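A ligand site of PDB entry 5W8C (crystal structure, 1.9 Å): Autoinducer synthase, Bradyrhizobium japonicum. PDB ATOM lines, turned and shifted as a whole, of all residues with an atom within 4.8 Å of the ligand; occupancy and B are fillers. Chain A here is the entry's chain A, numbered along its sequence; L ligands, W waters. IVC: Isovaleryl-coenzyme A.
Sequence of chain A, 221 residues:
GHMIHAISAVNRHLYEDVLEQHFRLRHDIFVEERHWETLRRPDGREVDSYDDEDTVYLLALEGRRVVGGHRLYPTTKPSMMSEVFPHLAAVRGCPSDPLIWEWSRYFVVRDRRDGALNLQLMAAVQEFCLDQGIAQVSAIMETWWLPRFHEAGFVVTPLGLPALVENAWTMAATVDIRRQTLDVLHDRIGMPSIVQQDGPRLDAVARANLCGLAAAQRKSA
Water W10 lies within hydrogen-bond range of O12 of the ligand (2.8 Å) and OD1 of Asp 114 (3.5 Å).
Water W9 bridges a nitrogen (N5) of the ligand (2.9 Å) and the guanidinium group of Arg 34 (3.5 Å).
Water W11 lies within hydrogen-bond range of O of Ile 140 (2.8 Å) and S1 of the ligand (3.0 Å).
Water W12 lies within hydrogen-bond range of a sulfur (S1) of the ligand (3.1 Å) and the indole nitrogen (NE1) of Trp 145 (3.4 Å).
O of Ile 29 sits at hydrogen-bond distance from N of Arg 34, at 2.9 Å.
OH of Tyr 106 lies within hydrogen-bond range of OD1 of Asn 118.
The guanidinium group of Arg 148 is in hydrogen-bond range of the side-chain amide oxygen of Asn 118.
The guanidinium group (NE) of Arg 113 lies within hydrogen-bond range of the backbone carbonyl oxygen (O) of Val 108.
The side-chain carboxylate (OE2) of Glu 33 is in salt-bridge range of the guanidinium group (NH1) of Arg 113.
The backbone carbonyl oxygen (O) of Phe 30 is in hydrogen-bond range of the backbone NH (N) of Trp 36, 2.9 Å away.
Ile 29 touches the ligand.
CE1 of Phe 30 touches N7 of the ligand, 3.6 Å away.
Trp 36 touches the ligand (CH2 to C21, 3.9 Å).
Trp 103 touches the ligand.
Ser 104 touches the ligand (C to O17, 3.6 Å).
Phe 107 touches the ligand (CA to O15, 3.4 Å).
Arg 113 touches the ligand.
Phe 149 touches the ligand (CZ to C26, 3.5 Å).
Hydrophobic or aromatic side chains within 4 Å of the ligand: Ile 29, Phe 30, Trp 36, Trp 103, Tyr 106, Phe 107, Val 108, Trp 144, Trp 145 and Phe 149.
Of the 23 residues printed, 17 come within 4 Å of the ligand.
The nearest printed residue that does not touch the ligand is Met 141 (4.03 Å).
An oxygen (O16) of the ligand lies within hydrogen-bond range of the guanidinium group (NH1) of Arg 34 (2.8 Å).
The backbone NH (N) of Tyr 106 lies within hydrogen-bond range of an oxygen (O17) of the ligand, at 3.0 Å.
N7 of the ligand lies within hydrogen-bond range of O of Tyr 106 (2.8 Å).
NH1 of Arg 148 is in salt-bridge range of O14 of the ligand, at 2.8 Å.
N of Val 108 lies within hydrogen-bond range of O15 of the ligand, 2.9 Å away.
The backbone NH (N) of Asp 114 sits at hydrogen-bond distance from an oxygen (O13) of the ligand (3.0 Å).
An oxygen (O17) of the ligand sits at hydrogen-bond distance from the backbone NH of Arg 105.
OD1 of Asn 118 lies close to O14 of the ligand, 3.5 Å away.
NE1 of Trp 145 lies close to S1 of the ligand.
NE1 of Trp 144 is in hydrogen-bond range of N4 of the ligand.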
ATOM      1  N   ILE A  29       7.514  -9.513  18.139  1.00  0.00           N
ATOM      2  CA  ILE A  29       8.915  -9.896  18.332  1.00  0.00           C
ATOM      3  C   ILE A  29       9.089 -11.134  19.202  1.00  0.00           C
ATOM      4  O   ILE A  29       9.732 -12.102  18.799  1.00  0.00           O
ATOM      5  CB  ILE A  29       9.754  -8.696  18.837  1.00  0.00           C
ATOM      6  CG1 ILE A  29       9.883  -7.649  17.717  1.00  0.00           C
ATOM      7  CG2 ILE A  29      11.133  -9.147  19.303  1.00  0.00           C
ATOM      8  CD1 ILE A  29      10.422  -6.306  18.165  1.00  0.00           C
ATOM      9  N   PHE A  30       8.508 -11.131  20.401  1.00  0.00           N
ATOM     10  CA  PHE A  30       8.704 -12.260  21.312  1.00  0.00           C
ATOM     11  C   PHE A  30       7.851 -13.480  20.969  1.00  0.00           C
ATOM     12  O   PHE A  30       8.287 -14.621  21.156  1.00  0.00           O
ATOM     13  CB  PHE A  30       8.559 -11.821  22.764  1.00  0.00           C
ATOM     14  CG  PHE A  30       9.618 -10.829  23.182  1.00  0.00           C
ATOM     15  CD1 PHE A  30      10.903 -11.262  23.469  1.00  0.00           C
ATOM     16  CD2 PHE A  30       9.333  -9.464  23.231  1.00  0.00           C
ATOM     17  CE1 PHE A  30      11.893 -10.362  23.837  1.00  0.00           C
ATOM     18  CE2 PHE A  30      10.314  -8.553  23.598  1.00  0.00           C
ATOM     19  CZ  PHE A  30      11.597  -9.004  23.898  1.00  0.00           C
ATOM     20  N   GLU A  33       8.445 -13.820  16.306  1.00  0.00           N
ATOM     21  CA  GLU A  33       9.852 -14.000  15.939  1.00  0.00           C
ATOM     22  C   GLU A  33      10.564 -15.024  16.833  1.00  0.00           C
ATOM     23  O   GLU A  33      11.112 -16.019  16.335  1.00  0.00           O
ATOM     24  CB  GLU A  33      10.625 -12.675  15.900  1.00  0.00           C
ATOM     25  CG  GLU A  33      12.093 -12.843  15.562  1.00  0.00           C
ATOM     26  CD  GLU A  33      12.907 -11.564  15.646  1.00  0.00           C
ATOM     27  OE1 GLU A  33      12.327 -10.473  15.845  1.00  0.00           O
ATOM     28  OE2 GLU A  33      14.142 -11.646  15.500  1.00  0.00           O
ATOM     29  N   ARG A  34      10.569 -14.780  18.140  1.00  0.00           N
ATOM     30  CA  ARG A  34      11.289 -15.672  19.057  1.00  0.00           C
ATOM     31  C   ARG A  34      10.543 -16.979  19.328  1.00  0.00           C
ATOM     32  O   ARG A  34      11.119 -17.929  19.848  1.00  0.00           O
ATOM     33  CB  ARG A  34      11.641 -14.959  20.368  1.00  0.00           C
ATOM     34  CG  ARG A  34      12.609 -13.791  20.240  1.00  0.00           C
ATOM     35  CD  ARG A  34      13.956 -14.156  19.623  1.00  0.00           C
ATOM     36  NE  ARG A  34      14.473 -15.426  20.118  1.00  0.00           N
ATOM     37  CZ  ARG A  34      15.174 -15.588  21.235  1.00  0.00           C
ATOM     38  NH1 ARG A  34      15.478 -14.536  21.997  1.00  0.00           N
ATOM     39  NH2 ARG A  34      15.581 -16.802  21.599  1.00  0.00           N
ATOM     40  N   TRP A  36       8.226 -17.529  21.525  1.00  0.00           N
ATOM     41  CA  TRP A  36       7.946 -17.741  22.937  1.00  0.00           C
ATOM     42  C   TRP A  36       6.441 -17.918  23.101  1.00  0.00           C
ATOM     43  O   TRP A  36       5.731 -17.018  23.565  1.00  0.00           O
ATOM     44  CB  TRP A  36       8.496 -16.611  23.809  1.00  0.00           C
ATOM     45  CG  TRP A  36      10.020 -16.541  23.831  1.00  0.00           C
ATOM     46  CD1 TRP A  36      10.894 -17.422  23.231  1.00  0.00           C
ATOM     47  CD2 TRP A  36      10.824 -15.578  24.517  1.00  0.00           C
ATOM     48  NE1 TRP A  36      12.192 -17.037  23.484  1.00  0.00           N
ATOM     49  CE2 TRP A  36      12.183 -15.923  24.275  1.00  0.00           C
ATOM     50  CE3 TRP A  36      10.539 -14.455  25.306  1.00  0.00           C
ATOM     51  CZ2 TRP A  36      13.242 -15.167  24.794  1.00  0.00           C
ATOM     52  CZ3 TRP A  36      11.593 -13.712  25.831  1.00  0.00           C
ATOM     53  CH2 TRP A  36      12.932 -14.073  25.568  1.00  0.00           C
ATOM     54  N   TRP A 103      15.101  -6.869  35.053  1.00  0.00           N
ATOM     55  CA  TRP A 103      15.268  -6.284  33.718  1.00  0.00           C
ATOM     56  C   TRP A 103      14.894  -7.329  32.665  1.00  0.00           C
ATOM     57  O   TRP A 103      15.434  -8.438  32.667  1.00  0.00           O
ATOM     58  CB  TRP A 103      16.728  -5.838  33.575  1.00  0.00           C
ATOM     59  CG  TRP A 103      17.067  -5.005  32.380  1.00  0.00           C
ATOM     60  CD1 TRP A 103      16.276  -4.052  31.791  1.00  0.00           C
ATOM     61  CD2 TRP A 103      18.300  -5.016  31.651  1.00  0.00           C
ATOM     62  NE1 TRP A 103      16.944  -3.492  30.725  1.00  0.00           N
ATOM     63  CE2 TRP A 103      18.187  -4.068  30.617  1.00  0.00           C
ATOM     64  CE3 TRP A 103      19.480  -5.756  31.766  1.00  0.00           C
ATOM     65  CZ2 TRP A 103      19.222  -3.821  29.700  1.00  0.00           C
ATOM     66  CZ3 TRP A 103      20.518  -5.515  30.856  1.00  0.00           C
ATOM     67  CH2 TRP A 103      20.369  -4.558  29.829  1.00  0.00           C
ATOM     68  N   SER A 104      13.964  -6.978  31.770  1.00  0.00           N
ATOM     69  CA  SER A 104      13.458  -7.938  30.780  1.00  0.00           C
ATOM     70  C   SER A 104      12.909  -7.283  29.516  1.00  0.00           C
ATOM     71  O   SER A 104      12.838  -6.048  29.423  1.00  0.00           O
ATOM     72  CB  SER A 104      12.358  -8.809  31.412  1.00  0.00           C
ATOM     73  OG  SER A 104      11.218  -8.021  31.738  1.00  0.00           O
ATOM     74  N   ARG A 105      12.523  -8.125  28.552  1.00  0.00           N
ATOM     75  CA  ARG A 105      11.864  -7.717  27.299  1.00  0.00           C
ATOM     76  C   ARG A 105      12.675  -6.708  26.481  1.00  0.00           C
ATOM     77  O   ARG A 105      12.127  -5.750  25.932  1.00  0.00           O
ATOM     78  CB  ARG A 105      10.430  -7.214  27.564  1.00  0.00           C
ATOM     79  CG  ARG A 105       9.475  -8.277  28.108  1.00  0.00           C
ATOM     80  CD  ARG A 105       9.270  -9.461  27.164  1.00  0.00           C
ATOM     81  NE  ARG A 105       8.023 -10.153  27.499  1.00  0.00           N
ATOM     82  CZ  ARG A 105       7.888 -11.043  28.481  1.00  0.00           C
ATOM     83  NH1 ARG A 105       8.929 -11.405  29.234  1.00  0.00           N
ATOM     84  NH2 ARG A 105       6.689 -11.577  28.714  1.00  0.00           N
ATOM     85  N   TYR A 106      13.978  -6.954  26.406  1.00  0.00           N
ATOM     86  CA  TYR A 106      14.911  -6.144  25.609  1.00  0.00           C
ATOM     87  C   TYR A 106      14.669  -6.439  24.131  1.00  0.00           C
ATOM     88  O   TYR A 106      14.712  -7.596  23.722  1.00  0.00           O
ATOM     89  CB  TYR A 106      16.327  -6.539  26.015  1.00  0.00           C
ATOM     90  CG  TYR A 106      17.465  -5.652  25.530  1.00  0.00           C
ATOM     91  CD1 TYR A 106      17.767  -5.506  24.176  1.00  0.00           C
ATOM     92  CD2 TYR A 106      18.302  -5.018  26.457  1.00  0.00           C
ATOM     93  CE1 TYR A 106      18.839  -4.723  23.750  1.00  0.00           C
ATOM     94  CE2 TYR A 106      19.369  -4.230  26.037  1.00  0.00           C
ATOM     95  CZ  TYR A 106      19.636  -4.091  24.690  1.00  0.00           C
ATOM     96  OH  TYR A 106      20.695  -3.315  24.289  1.00  0.00           O
ATOM     97  N   PHE A 107      14.406  -5.400  23.345  1.00  0.00           N
ATOM     98  CA  PHE A 107      14.192  -5.591  21.900  1.00  0.00           C
ATOM     99  C   PHE A 107      14.654  -4.381  21.089  1.00  0.00           C
ATOM    100  O   PHE A 107      14.707  -3.260  21.583  1.00  0.00           O
ATOM    101  CB  PHE A 107      12.725  -5.921  21.592  1.00  0.00           C
ATOM    102  CG  PHE A 107      11.793  -4.741  21.748  1.00  0.00           C
ATOM    103  CD1 PHE A 107      11.269  -4.409  22.994  1.00  0.00           C
ATOM    104  CD2 PHE A 107      11.430  -3.967  20.648  1.00  0.00           C
ATOM    105  CE1 PHE A 107      10.423  -3.324  23.148  1.00  0.00           C
ATOM    106  CE2 PHE A 107      10.571  -2.893  20.784  1.00  0.00           C
ATOM    107  CZ  PHE A 107      10.064  -2.566  22.034  1.00  0.00           C
ATOM    108  N   VAL A 108      14.994  -4.655  19.835  1.00  0.00           N
ATOM    109  CA  VAL A 108      15.268  -3.639  18.840  1.00  0.00           C
ATOM    110  C   VAL A 108      14.500  -4.085  17.598  1.00  0.00           C
ATOM    111  O   VAL A 108      14.599  -5.253  17.201  1.00  0.00           O
ATOM    112  CB  VAL A 108      16.782  -3.540  18.528  1.00  0.00           C
ATOM    113  CG1 VAL A 108      17.053  -2.606  17.346  1.00  0.00           C
ATOM    114  CG2 VAL A 108      17.555  -3.057  19.744  1.00  0.00           C
ATOM    115  N   ARG A 112      16.288  -1.266  12.956  1.00  0.00           N
ATOM    116  CA  ARG A 112      17.335  -0.600  13.728  1.00  0.00           C
ATOM    117  C   ARG A 112      18.379  -1.532  14.324  1.00  0.00           C
ATOM    118  O   ARG A 112      19.192  -1.113  15.138  1.00  0.00           O
ATOM    119  CB  ARG A 112      16.709   0.269  14.833  1.00  0.00           C
ATOM    120  CG  ARG A 112      15.884   1.452  14.337  1.00  0.00           C
ATOM    121  CD  ARG A 112      16.753   2.497  13.635  1.00  0.00           C
ATOM    122  NE  ARG A 112      15.940   3.590  13.116  1.00  0.00           N
ATOM    123  CZ  ARG A 112      15.393   3.635  11.902  1.00  0.00           C
ATOM    124  NH1 ARG A 112      15.577   2.634  11.048  1.00  0.00           N
ATOM    125  NH2 ARG A 112      14.676   4.682  11.538  1.00  0.00           N
ATOM    126  N   ARG A 113      18.355  -2.807  13.922  1.00  0.00           N
ATOM    127  CA  ARG A 113      19.322  -3.778  14.432  1.00  0.00           C
ATOM    128  C   ARG A 113      20.696  -3.580  13.783  1.00  0.00           C
ATOM    129  O   ARG A 113      20.797  -3.055  12.677  1.00  0.00           O
ATOM    130  CB  ARG A 113      18.825  -5.208  14.221  1.00  0.00           C
ATOM    131  CG  ARG A 113      17.647  -5.545  15.115  1.00  0.00           C
ATOM    132  CD  ARG A 113      17.154  -6.969  14.920  1.00  0.00           C
ATOM    133  NE  ARG A 113      15.873  -7.142  15.583  1.00  0.00           N
ATOM    134  CZ  ARG A 113      15.166  -8.261  15.606  1.00  0.00           C
ATOM    135  NH1 ARG A 113      15.613  -9.352  14.986  1.00  0.00           N
ATOM    136  NH2 ARG A 113      14.000  -8.289  16.239  1.00  0.00           N
ATOM    137  N   ASP A 114      21.738  -3.999  14.503  1.00  0.00           N
ATOM    138  CA  ASP A 114      23.125  -3.886  14.048  1.00  0.00           C
ATOM    139  C   ASP A 114      23.498  -2.427  13.726  1.00  0.00           C
ATOM    140  O   ASP A 114      24.186  -2.143  12.749  1.00  0.00           O
ATOM    141  CB  ASP A 114      23.392  -4.825  12.853  1.00  0.00           C
ATOM    142  CG  ASP A 114      24.872  -4.965  12.533  1.00  0.00           C
ATOM    143  OD1 ASP A 114      25.710  -4.904  13.462  1.00  0.00           O
ATOM    144  OD2 ASP A 114      25.196  -5.139  11.340  1.00  0.00           O
ATOM    145  N   GLY A 115      23.007  -1.504  14.558  1.00  0.00           N
ATOM    146  CA  GLY A 115      23.279  -0.075  14.408  1.00  0.00           C
ATOM    147  C   GLY A 115      23.654   0.532  15.746  1.00  0.00           C
ATOM    148  O   GLY A 115      24.159  -0.151  16.629  1.00  0.00           O
ATOM    149  N   ASN A 118      21.453  -0.364  19.747  1.00  0.00           N
ATOM    150  CA  ASN A 118      21.704  -1.381  20.756  1.00  0.00           C
ATOM    151  C   ASN A 118      22.552  -0.881  21.931  1.00  0.00           C
ATOM    152  O   ASN A 118      22.186  -1.094  23.092  1.00  0.00           O
ATOM    153  CB  ASN A 118      22.328  -2.647  20.171  1.00  0.00           C
ATOM    154  CG  ASN A 118      22.481  -3.732  21.213  1.00  0.00           C
ATOM    155  OD1 ASN A 118      21.493  -4.240  21.740  1.00  0.00           O
ATOM    156  ND2 ASN A 118      23.729  -4.065  21.541  1.00  0.00           N
ATOM    157  N   ALA A 139      18.277 -10.418  35.983  1.00  0.00           N
ATOM    158  CA  ALA A 139      17.702 -10.857  34.719  1.00  0.00           C
ATOM    159  C   ALA A 139      17.742 -12.355  34.528  1.00  0.00           C
ATOM    160  O   ALA A 139      18.649 -13.038  35.014  1.00  0.00           O
ATOM    161  CB  ALA A 139      18.408 -10.163  33.561  1.00  0.00           C
ATOM    162  N   ILE A 140      16.744 -12.873  33.819  1.00  0.00           N
ATOM    163  CA  ILE A 140      16.786 -14.220  33.282  1.00  0.00           C
ATOM    164  C   ILE A 140      17.087 -14.079  31.805  1.00  0.00           C
ATOM    165  O   ILE A 140      16.275 -13.547  31.055  1.00  0.00           O
ATOM    166  CB  ILE A 140      15.431 -14.941  33.432  1.00  0.00           C
ATOM    167  CG1 ILE A 140      15.013 -15.010  34.902  1.00  0.00           C
ATOM    168  CG2 ILE A 140      15.498 -16.322  32.804  1.00  0.00           C
ATOM    169  CD1 ILE A 140      14.279 -13.776  35.366  1.00  0.00           C
ATOM    170  N   MET A 141      18.267 -14.530  31.378  1.00  0.00           N
ATOM    171  CA  MET A 141      18.650 -14.356  29.979  1.00  0.00           C
ATOM    172  C   MET A 141      19.308 -15.591  29.368  1.00  0.00           C
ATOM    173  O   MET A 141      19.946 -16.381  30.063  1.00  0.00           O
ATOM    174  CB  MET A 141      19.586 -13.152  29.824  1.00  0.00           C
ATOM    175  CG  MET A 141      21.041 -13.437  30.157  1.00  0.00           C
ATOM    176  SD  MET A 141      21.367 -13.606  31.924  1.00  0.00           S
ATOM    177  CE  MET A 141      23.130 -13.315  31.961  1.00  0.00           C
ATOM    178  N   TRP A 144      23.727 -16.504  25.378  1.00  0.00           N
ATOM    179  CA  TRP A 144      24.361 -15.657  24.344  1.00  0.00           C
ATOM    180  C   TRP A 144      24.482 -14.194  24.757  1.00  0.00           C
ATOM    181  O   TRP A 144      25.207 -13.423  24.122  1.00  0.00           O
ATOM    182  CB  TRP A 144      23.697 -15.821  22.961  1.00  0.00           C
ATOM    183  CG  TRP A 144      22.206 -15.563  22.886  1.00  0.00           C
ATOM    184  CD1 TRP A 144      21.208 -16.504  22.957  1.00  0.00           C
ATOM    185  CD2 TRP A 144      21.555 -14.301  22.674  1.00  0.00           C
ATOM    186  NE1 TRP A 144      19.983 -15.897  22.817  1.00  0.00           N
ATOM    187  CE2 TRP A 144      20.157 -14.551  22.647  1.00  0.00           C
ATOM    188  CE3 TRP A 144      22.008 -12.987  22.513  1.00  0.00           C
ATOM    189  CZ2 TRP A 144      19.216 -13.527  22.464  1.00  0.00           C
ATOM    190  CZ3 TRP A 144      21.067 -11.963  22.330  1.00  0.00           C
ATOM    191  CH2 TRP A 144      19.681 -12.248  22.311  1.00  0.00           C
ATOM    192  N   TRP A 145      23.798 -13.812  25.833  1.00  0.00           N
ATOM    193  CA  TRP A 145      23.935 -12.465  26.373  1.00  0.00           C
ATOM    194  C   TRP A 145      25.262 -12.190  27.075  1.00  0.00           C
ATOM    195  O   TRP A 145      25.658 -11.020  27.205  1.00  0.00           O
ATOM    196  CB  TRP A 145      22.781 -12.151  27.334  1.00  0.00           C
ATOM    197  CG  TRP A 145      21.581 -11.646  26.620  1.00  0.00           C
ATOM    198  CD1 TRP A 145      20.525 -12.376  26.161  1.00  0.00           C
ATOM    199  CD2 TRP A 145      21.322 -10.288  26.254  1.00  0.00           C
ATOM    200  NE1 TRP A 145      19.606 -11.548  25.544  1.00  0.00           N
ATOM    201  CE2 TRP A 145      20.075 -10.262  25.595  1.00  0.00           C
ATOM    202  CE3 TRP A 145      22.023  -9.081  26.438  1.00  0.00           C
ATOM    203  CZ2 TRP A 145      19.507  -9.082  25.113  1.00  0.00           C
ATOM    204  CZ3 TRP A 145      21.457  -7.907  25.964  1.00  0.00           C
ATOM    205  CH2 TRP A 145      20.211  -7.916  25.303  1.00  0.00           C
ATOM    206  N   ARG A 148      27.706 -10.144  25.128  1.00  0.00           N
ATOM    207  CA  ARG A 148      27.106  -8.818  24.924  1.00  0.00           C
ATOM    208  C   ARG A 148      27.258  -7.953  26.163  1.00  0.00           C
ATOM    209  O   ARG A 148      27.607  -6.779  26.072  1.00  0.00           O
ATOM    210  CB  ARG A 148      25.641  -8.946  24.512  1.00  0.00           C
ATOM    211  CG  ARG A 148      25.452  -9.314  23.048  1.00  0.00           C
ATOM    212  CD  ARG A 148      24.024  -9.758  22.726  1.00  0.00           C
ATOM    213  NE  ARG A 148      23.002  -8.738  22.998  1.00  0.00           N
ATOM    214  CZ  ARG A 148      22.678  -7.739  22.174  1.00  0.00           C
ATOM    215  NH1 ARG A 148      23.305  -7.580  21.009  1.00  0.00           N
ATOM    216  NH2 ARG A 148      21.708  -6.894  22.512  1.00  0.00           N
ATOM    217  N   PHE A 149      27.013  -8.533  27.343  1.00  0.00           N
ATOM    218  CA  PHE A 149      27.239  -7.822  28.604  1.00  0.00           C
ATOM    219  C   PHE A 149      28.701  -7.426  28.741  1.00  0.00           C
ATOM    220  O   PHE A 149      29.011  -6.295  29.111  1.00  0.00           O
ATOM    221  CB  PHE A 149      26.834  -8.686  29.797  1.00  0.00           C
ATOM    222  CG  PHE A 149      25.357  -8.784  30.016  1.00  0.00           C
ATOM    223  CD1 PHE A 149      24.479  -7.908  29.396  1.00  0.00           C
ATOM    224  CD2 PHE A 149      24.839  -9.739  30.881  1.00  0.00           C
ATOM    225  CE1 PHE A 149      23.117  -7.984  29.605  1.00  0.00           C
ATOM    226  CE2 PHE A 149      23.468  -9.811  31.110  1.00  0.00           C
ATOM    227  CZ  PHE A 149      22.612  -8.939  30.466  1.00  0.00           C
HETATM  228  O9  IVC L   1      23.838 -12.367  14.097  1.00  0.00           O
HETATM  229  P1  IVC L   1      25.252 -12.199  14.587  1.00  0.00           P
HETATM  230  O5  IVC L   1      26.151 -11.458  13.627  1.00  0.00           O
HETATM  231  O6  IVC L   1      25.862 -13.453  15.168  1.00  0.00           O
HETATM  232  O2  IVC L   1      25.184 -11.186  15.838  1.00  0.00           O
HETATM  233  C1  IVC L   1      24.134 -11.263  16.805  1.00  0.00           C
HETATM  234  C2  IVC L   1      24.237 -12.480  17.690  1.00  0.00           C
HETATM  235  O3  IVC L   1      25.612 -12.756  18.006  1.00  0.00           O
HETATM  236  C4  IVC L   1      23.546 -12.040  18.964  1.00  0.00           C
HETATM  237  N1  IVC L   1      22.122 -12.500  18.962  1.00  0.00           N
HETATM  238  C7  IVC L   1      21.032 -11.736  18.782  1.00  0.00           C
HETATM  239  N2  IVC L   1      19.940 -12.525  18.862  1.00  0.00           N
HETATM  240  C8  IVC L   1      20.352 -13.784  19.095  1.00  0.00           C
HETATM  241  C6  IVC L   1      21.736 -13.762  19.155  1.00  0.00           C
HETATM  242  N3  IVC L   1      22.431 -14.901  19.385  1.00  0.00           N
HETATM  243  C15 IVC L   1      21.779 -16.061  19.555  1.00  0.00           C
HETATM  244  N4  IVC L   1      20.435 -16.116  19.494  1.00  0.00           N
HETATM  245  C12 IVC L   1      19.706 -15.001  19.269  1.00  0.00           C
HETATM  246  N5  IVC L   1      18.351 -15.081  19.219  1.00  0.00           N
HETATM  247  O1  IVC L   1      23.602 -10.610  18.998  1.00  0.00           O
HETATM  248  C3  IVC L   1      24.233 -10.126  17.803  1.00  0.00           C
HETATM  249  C5  IVC L   1      23.588  -8.833  17.332  1.00  0.00           C
HETATM  250  O4  IVC L   1      22.197  -9.037  17.099  1.00  0.00           O
HETATM  251  P2  IVC L   1      21.420  -8.134  16.025  1.00  0.00           P
HETATM  252  O12 IVC L   1      22.155  -8.247  14.708  1.00  0.00           O
HETATM  253  O10 IVC L   1      19.957  -8.505  16.056  1.00  0.00           O
HETATM  254  O7  IVC L   1      21.695  -6.629  16.511  1.00  0.00           O
HETATM  255  P3  IVC L   1      21.292  -5.811  17.842  1.00  0.00           P
HETATM  256  O14 IVC L   1      22.391  -5.954  18.860  1.00  0.00           O
HETATM  257  O13 IVC L   1      20.949  -4.420  17.358  1.00  0.00           O
HETATM  258  O8  IVC L   1      19.929  -6.488  18.377  1.00  0.00           O
HETATM  259  C11 IVC L   1      19.970  -7.561  19.322  1.00  0.00           C
HETATM  260  C9  IVC L   1      18.569  -7.881  19.842  1.00  0.00           C
HETATM  261  C13 IVC L   1      18.632  -9.149  20.686  1.00  0.00           C
HETATM  262  C14 IVC L   1      18.114  -6.716  20.712  1.00  0.00           C
HETATM  263  C10 IVC L   1      17.614  -8.047  18.641  1.00  0.00           C
HETATM  264  O11 IVC L   1      18.060  -9.071  17.742  1.00  0.00           O
HETATM  265  C16 IVC L   1      16.190  -8.361  19.040  1.00  0.00           C
HETATM  266  O15 IVC L   1      15.425  -7.455  19.354  1.00  0.00           O
HETATM  267  N6  IVC L   1      15.817  -9.638  18.989  1.00  0.00           N
HETATM  268  C17 IVC L   1      14.502 -10.205  19.316  1.00  0.00           C
HETATM  269  C18 IVC L   1      14.220  -9.952  20.800  1.00  0.00           C
HETATM  270  C19 IVC L   1      15.130 -10.749  21.700  1.00  0.00           C
HETATM  271  O16 IVC L   1      15.625 -11.805  21.332  1.00  0.00           O
HETATM  272  N7  IVC L   1      15.348 -10.250  22.925  1.00  0.00           N
HETATM  273  C20 IVC L   1      16.189 -10.848  23.945  1.00  0.00           C
HETATM  274  C21 IVC L   1      15.330 -10.991  25.205  1.00  0.00           C
HETATM  275  S1  IVC L   1      16.424 -11.296  26.560  1.00  0.00           S
HETATM  276  C22 IVC L   1      16.188 -10.141  27.746  1.00  0.00           C
HETATM  277  O17 IVC L   1      15.270  -9.329  27.650  1.00  0.00           O
HETATM  278  C23 IVC L   1      17.110 -10.097  28.939  1.00  0.00           C
HETATM  279  C24 IVC L   1      17.928  -8.814  28.850  1.00  0.00           C
HETATM  280  C25 IVC L   1      17.260  -7.699  29.648  1.00  0.00           C
HETATM  281  C26 IVC L   1      19.346  -9.068  29.329  1.00  0.00           C
HETATM  282  O   HOH W   1      25.146 -15.591  19.247  1.00  0.00           O
HETATM  283  O   HOH W   2      17.207 -12.382  18.948  1.00  0.00           O
HETATM  284  O   HOH W   3      27.104 -10.770  20.176  1.00  0.00           O
HETATM  285  O   HOH W   4      21.096  -7.640  12.167  1.00  0.00           O
HETATM  286  O   HOH W   5      25.973  -7.952  19.850  1.00  0.00           O
HETATM  287  O   HOH W   6      21.746 -10.713  13.379  1.00  0.00           O
HETATM  288  O   HOH W   7      21.175  -1.733  17.005  1.00  0.00           O
HETATM  289  O   HOH W   8      27.611 -14.262  19.801  1.00  0.00           O
HETATM  290  O   HOH W   9      17.183 -17.635  18.624  1.00  0.00           O
HETATM  291  O   HOH W  10      24.709  -8.214  13.584  1.00  0.00           O
HETATM  292  O   HOH W  11      14.891 -12.547  28.844  1.00  0.00           O
HETATM  293  O   HOH W  12      17.248 -13.957  25.130  1.00  0.00           O
HETATM  294  O   HOH W  13      26.544  -7.123  17.031  1.00  0.00           O
HETATM  295  O   HOH W  14      24.813  -4.994  18.177  1.00  0.00           O
HETATM  296  O   HOH W  15      20.152 -18.774  20.119  1.00  0.00           O
HETATM  297  O   HOH W  16      27.960 -10.719  17.263  1.00  0.00           O
